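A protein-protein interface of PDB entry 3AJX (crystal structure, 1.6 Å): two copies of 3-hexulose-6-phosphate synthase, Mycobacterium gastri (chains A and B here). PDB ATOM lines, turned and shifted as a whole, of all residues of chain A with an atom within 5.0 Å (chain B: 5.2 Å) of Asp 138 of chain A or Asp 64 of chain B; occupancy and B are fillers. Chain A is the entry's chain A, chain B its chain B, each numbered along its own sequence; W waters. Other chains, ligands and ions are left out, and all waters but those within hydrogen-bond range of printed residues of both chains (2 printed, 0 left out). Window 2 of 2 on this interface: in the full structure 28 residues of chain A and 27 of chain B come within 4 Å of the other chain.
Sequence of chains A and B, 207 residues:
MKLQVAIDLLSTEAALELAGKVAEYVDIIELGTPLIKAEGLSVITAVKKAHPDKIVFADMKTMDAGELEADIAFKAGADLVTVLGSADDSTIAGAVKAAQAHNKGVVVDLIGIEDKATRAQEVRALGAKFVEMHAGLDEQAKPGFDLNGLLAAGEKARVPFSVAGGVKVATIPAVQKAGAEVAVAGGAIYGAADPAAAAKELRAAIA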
ATOM      1  N   ILE A 111      -7.815  -4.815  14.390  1.00  0.00           N
ATOM      2  CA  ILE A 111      -8.615  -5.654  15.272  1.00  0.00           C
ATOM      3  C   ILE A 111      -9.514  -6.581  14.445  1.00  0.00           C
ATOM      4  O   ILE A 111     -10.112  -6.164  13.449  1.00  0.00           O
ATOM      5  CB  ILE A 111      -9.489  -4.781  16.215  1.00  0.00           C
ATOM      6  CG1 ILE A 111     -10.262  -5.666  17.195  1.00  0.00           C
ATOM      7  CG2 ILE A 111     -10.448  -3.929  15.399  1.00  0.00           C
ATOM      8  CD1 ILE A 111     -10.962  -4.888  18.298  1.00  0.00           C
ATOM      9  N   GLY A 136      -9.079  -6.866  20.887  1.00  0.00           N
ATOM     10  CA  GLY A 136     -10.103  -6.220  21.688  1.00  0.00           C
ATOM     11  C   GLY A 136     -10.368  -6.875  23.029  1.00  0.00           C
ATOM     12  O   GLY A 136      -9.817  -7.929  23.343  1.00  0.00           O
ATOM     13  N   LEU A 137     -11.231  -6.249  23.822  1.00  0.00           N
ATOM     14  CA  LEU A 137     -11.572  -6.773  25.138  1.00  0.00           C
ATOM     15  C   LEU A 137     -12.254  -8.136  25.062  1.00  0.00           C
ATOM     16  O   LEU A 137     -12.004  -9.004  25.898  1.00  0.00           O
ATOM     17  CB  LEU A 137     -12.461  -5.778  25.889  1.00  0.00           C
ATOM     18  CG  LEU A 137     -11.818  -4.415  26.171  1.00  0.00           C
ATOM     19  CD1 LEU A 137     -12.807  -3.519  26.897  1.00  0.00           C
ATOM     20  CD2 LEU A 137     -10.554  -4.598  27.009  1.00  0.00           C
ATOM     21  N   ASP A 138     -13.109  -8.341  24.066  1.00  0.00           N
ATOM     22  CA  ASP A 138     -13.778  -9.631  23.948  1.00  0.00           C
ATOM     23  C   ASP A 138     -12.787 -10.735  23.602  1.00  0.00           C
ATOM     24  O   ASP A 138     -12.877 -11.845  24.130  1.00  0.00           O
ATOM     25  CB  ASP A 138     -14.895  -9.569  22.902  1.00  0.00           C
ATOM     26  CG  ASP A 138     -16.085  -8.752  23.373  1.00  0.00           C
ATOM     27  OD1 ASP A 138     -16.470  -8.898  24.552  1.00  0.00           O
ATOM     28  OD2 ASP A 138     -16.640  -7.976  22.570  1.00  0.00           O
ATOM     29  N   GLU A 139     -11.833 -10.431  22.726  1.00  0.00           N
ATOM     30  CA  GLU A 139     -10.832 -11.417  22.334  1.00  0.00           C
ATOM     31  C   GLU A 139      -9.902 -11.731  23.503  1.00  0.00           C
ATOM     32  O   GLU A 139      -9.513 -12.883  23.713  1.00  0.00           O
ATOM     33  CB  GLU A 139     -10.012 -10.903  21.146  1.00  0.00           C
ATOM     34  CG  GLU A 139      -8.867 -11.828  20.755  1.00  0.00           C
ATOM     35  CD  GLU A 139      -8.128 -11.371  19.515  1.00  0.00           C
ATOM     36  OE1 GLU A 139      -7.139 -12.039  19.144  1.00  0.00           O
ATOM     37  OE2 GLU A 139      -8.533 -10.355  18.908  1.00  0.00           O
ATOM     38  N   GLN A 140      -9.551 -10.699  24.263  1.00  0.00           N
ATOM     39  CA  GLN A 140      -8.667 -10.855  25.413  1.00  0.00           C
ATOM     40  C   GLN A 140      -9.292 -11.759  26.467  1.00  0.00           C
ATOM     41  O   GLN A 140      -8.588 -12.469  27.184  1.00  0.00           O
ATOM     42  CB  GLN A 140      -8.369  -9.492  26.044  1.00  0.00           C
ATOM     43  CG  GLN A 140      -7.455  -8.594  25.230  1.00  0.00           C
ATOM     44  CD  GLN A 140      -7.266  -7.231  25.873  1.00  0.00           C
ATOM     45  OE1 GLN A 140      -6.930  -7.130  27.054  1.00  0.00           O
ATOM     46  NE2 GLN A 140      -7.481  -6.176  25.098  1.00  0.00           N
ATOM     47  N   ALA A 141     -10.619 -11.727  26.550  1.00  0.00           N
ATOM     48  CA  ALA A 141     -11.358 -12.518  27.526  1.00  0.00           C
ATOM     49  C   ALA A 141     -11.376 -14.011  27.223  1.00  0.00           C
ATOM     50  O   ALA A 141     -11.665 -14.820  28.106  1.00  0.00           O
ATOM     51  CB  ALA A 141     -12.785 -11.993  27.636  1.00  0.00           C
ATOM     52  N   LYS A 142     -11.081 -14.382  25.983  1.00  0.00           N
ATOM     53  CA  LYS A 142     -11.078 -15.790  25.612  1.00  0.00           C
ATOM     54  C   LYS A 142      -9.949 -16.529  26.317  1.00  0.00           C
ATOM     55  O   LYS A 142      -8.815 -16.051  26.369  1.00  0.00           O
ATOM     56  CB  LYS A 142     -10.933 -15.950  24.098  1.00  0.00           C
ATOM     57  CG  LYS A 142     -12.129 -15.453  23.307  1.00  0.00           C
ATOM     58  CD  LYS A 142     -11.989 -15.780  21.831  1.00  0.00           C
ATOM     59  CE  LYS A 142     -13.243 -15.389  21.068  1.00  0.00           C
ATOM     60  NZ  LYS A 142     -13.181 -15.806  19.640  1.00  0.00           N
ATOM     61  N   THR B  62     -20.757  -1.796  16.079  1.00  0.00           N
ATOM     62  CA  THR B  62     -19.848  -2.253  17.119  1.00  0.00           C
ATOM     63  C   THR B  62     -18.828  -3.255  16.592  1.00  0.00           C
ATOM     64  O   THR B  62     -19.175  -4.183  15.865  1.00  0.00           O
ATOM     65  CB  THR B  62     -20.644  -2.894  18.268  1.00  0.00           C
ATOM     66  OG1 THR B  62     -21.596  -1.945  18.762  1.00  0.00           O
ATOM     67  CG2 THR B  62     -19.719  -3.316  19.406  1.00  0.00           C
ATOM     68  N   MET B  63     -17.565  -3.055  16.969  1.00  0.00           N
ATOM     69  CA  MET B  63     -16.479  -3.933  16.544  1.00  0.00           C
ATOM     70  C   MET B  63     -15.831  -4.639  17.738  1.00  0.00           C
ATOM     71  O   MET B  63     -15.105  -5.621  17.572  1.00  0.00           O
ATOM     72  CB  MET B  63     -15.431  -3.125  15.773  1.00  0.00           C
ATOM     73  CG  MET B  63     -14.330  -3.957  15.136  1.00  0.00           C
ATOM     74  SD  MET B  63     -14.935  -5.261  14.033  1.00  0.00           S
ATOM     75  CE  MET B  63     -13.579  -6.457  14.188  1.00  0.00           C
ATOM     76  N   ASP B  64     -16.097  -4.137  18.940  1.00  0.00           N
ATOM     77  CA  ASP B  64     -15.552  -4.728  20.163  1.00  0.00           C
ATOM     78  C   ASP B  64     -16.387  -4.308  21.370  1.00  0.00           C
ATOM     79  O   ASP B  64     -17.096  -3.299  21.323  1.00  0.00           O
ATOM     80  CB  ASP B  64     -14.089  -4.307  20.355  1.00  0.00           C
ATOM     81  CG  ASP B  64     -13.437  -4.984  21.550  1.00  0.00           C
ATOM     82  OD1 ASP B  64     -13.646  -6.205  21.728  1.00  0.00           O
ATOM     83  OD2 ASP B  64     -12.710  -4.301  22.304  1.00  0.00           O
ATOM     84  N   ALA B  65     -16.294  -5.083  22.449  1.00  0.00           N
ATOM     85  CA  ALA B  65     -17.061  -4.814  23.663  1.00  0.00           C
ATOM     86  C   ALA B  65     -18.538  -4.830  23.289  1.00  0.00           C
ATOM     87  O   ALA B  65     -19.273  -3.871  23.538  1.00  0.00           O
ATOM     88  CB  ALA B  65     -16.672  -3.461  24.251  1.00  0.00           C
ATOM     89  N   GLY B  66     -18.958  -5.939  22.685  1.00  0.00           N
ATOM     90  CA  GLY B  66     -20.330  -6.093  22.243  1.00  0.00           C
ATOM     91  C   GLY B  66     -21.395  -5.788  23.276  1.00  0.00           C
ATOM     92  O   GLY B  66     -22.317  -5.017  23.013  1.00  0.00           O
ATOM     93  N   GLU B  69     -21.372  -1.789  24.275  1.00  0.00           N
ATOM     94  CA  GLU B  69     -21.971  -0.876  23.305  1.00  0.00           C
ATOM     95  C   GLU B  69     -23.468  -1.100  23.147  1.00  0.00           C
ATOM     96  O   GLU B  69     -24.226  -0.140  23.010  1.00  0.00           O
ATOM     97  CB  GLU B  69     -21.264  -0.984  21.948  1.00  0.00           C
ATOM     98  CG  GLU B  69     -19.820  -0.491  22.002  1.00  0.00           C
ATOM     99  CD  GLU B  69     -19.311   0.043  20.673  1.00  0.00           C
ATOM    100  OE1 GLU B  69     -20.088   0.084  19.695  1.00  0.00           O
ATOM    101  OE2 GLU B  69     -18.120   0.429  20.614  1.00  0.00           O
ATOM    102  N   SER B  90     -17.644 -13.611  19.675  1.00  0.00           N
ATOM    103  CA  SER B  90     -17.892 -13.273  21.074  1.00  0.00           C
ATOM    104  C   SER B  90     -18.427 -11.854  21.241  1.00  0.00           C
ATOM    105  O   SER B  90     -19.157 -11.571  22.188  1.00  0.00           O
ATOM    106  CB  SER B  90     -16.616 -13.448  21.906  1.00  0.00           C
ATOM    107  OG  SER B  90     -15.594 -12.556  21.500  1.00  0.00           O
ATOM    108  N   THR B  91     -18.055 -10.959  20.328  1.00  0.00           N
ATOM    109  CA  THR B  91     -18.533  -9.582  20.390  1.00  0.00           C
ATOM    110  C   THR B  91     -20.014  -9.566  20.012  1.00  0.00           C
ATOM    111  O   THR B  91     -20.815  -8.855  20.624  1.00  0.00           O
ATOM    112  CB  THR B  91     -17.741  -8.674  19.430  1.00  0.00           C
ATOM    113  OG1 THR B  91     -16.372  -8.614  19.853  1.00  0.00           O
ATOM    114  CG2 THR B  91     -18.324  -7.261  19.421  1.00  0.00           C
HETATM  115  O   HOH W   1     -19.000  -8.283  25.196  1.00  0.00           O
HETATM  116  O   HOH W   2     -12.446  -8.415  20.738  1.00  0.00           O
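Among the printed residues, pairs that only touch across the chains: Ile 111 of chain A with Met 63 of chain B (3.6 Å), Ile 111 of chain A with Asp 64 of chain B (3.8 Å), Gly 136 of chain A with Asp 64 of chain B (3.3 Å), Asp 138 of chain A with Ser 90 of chain B (3.4 Å) and Lys 142 of chain A with Ser 90 of chain B (3.7 Å).
Water W1 lies within hydrogen-bond range of the side-chain carboxylate (OD1) of Asp 138 of chain A and the backbone NH (N) of Gly 66 of chain B.
Water W2 lies within hydrogen-bond range of OD1 of Asp 64 of chain B, N of Glu 139 of chain A and N of Asp 138 of chain A.
The backbone NH (N) of Leu 137 of chain A lies within hydrogen-bond range of the side-chain carboxylate (OD2) of Asp 64 of chain B, at 2.9 Å.
The side-chain carboxylate of Asp 138 of chain A is in hydrogen-bond range of the backbone NH of Ala 65 of chain B (2.9 Å).
OD2 of Asp 138 of chain A sits at hydrogen-bond distance from N of Gly 66 of chain B (3.1 Å).
N of Asp 138 of chain A sits at hydrogen-bond distance from OD1 of Asp 64 of chain B (3.2 Å).
The side-chain carboxylate (OD2) of Asp 138 of chain A lies within hydrogen-bond range of the side-chain hydroxyl (OG1) of Thr 91 of chain B, 2.8 Å away.
No position is printed for both chains.
Of the 10 pairs that touch across the chains among the printed residues, none has its exchanged pair printed and touching as well.
Of the printed residues of chain B, Gly 136 of chain A touches Asp 64 (3.3 Å).
Of chain B, only Asp 64 (3.2 Å), Ala 65 (2.9 Å), Gly 66 (3.1 Å), Ser 90 (3.4 Å) and Thr 91 (2.8 Å) come within 4 Å of Asp 138 of chain A.
Glu 139 of chain A touches none of the printed residues of chain B.
Thr 62 of chain B touches none of the printed residues of chain A.
Of the printed residues of chain A, Met 63 of chain B touches Ile 111 (3.6 Å).
Asp 64 of chain B touches just these residues of chain A: Ile 111, Gly 136, Leu 137 and Asp 138.
Of the printed residues of chain A, Ala 65 of chain B touches Asp 138 (2.9 Å).
The nearest residue of chain A that does not touch Asp 64 of chain B is Glu 139 of chain A (4.7 Å).
The nearest printed residue of chain A that does not touch Met 63 of chain B is Asp 138 of chain A (5.7 Å).
O of Gly 136 of chain A lies close to NE2 of Gln 140 of chain A (3.4 Å).
Of the 8 printed residues of chain B, 6 touch a printed residue of chain A.
Hydrophobic or aromatic side chains of chain B within 4 Å of the printed part of chain A: Met 63.
Printed residues of chain A that touch a printed residue of chain B: Ile 111, Gly 136, Leu 137, Asp 138 and Lys 142.
Hydrophobic or aromatic side chains of chain A within 4 Å of the printed part of chain B: Ile 111 and Leu 137.
Among the printed residues, 10 pairs touch across the chains.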
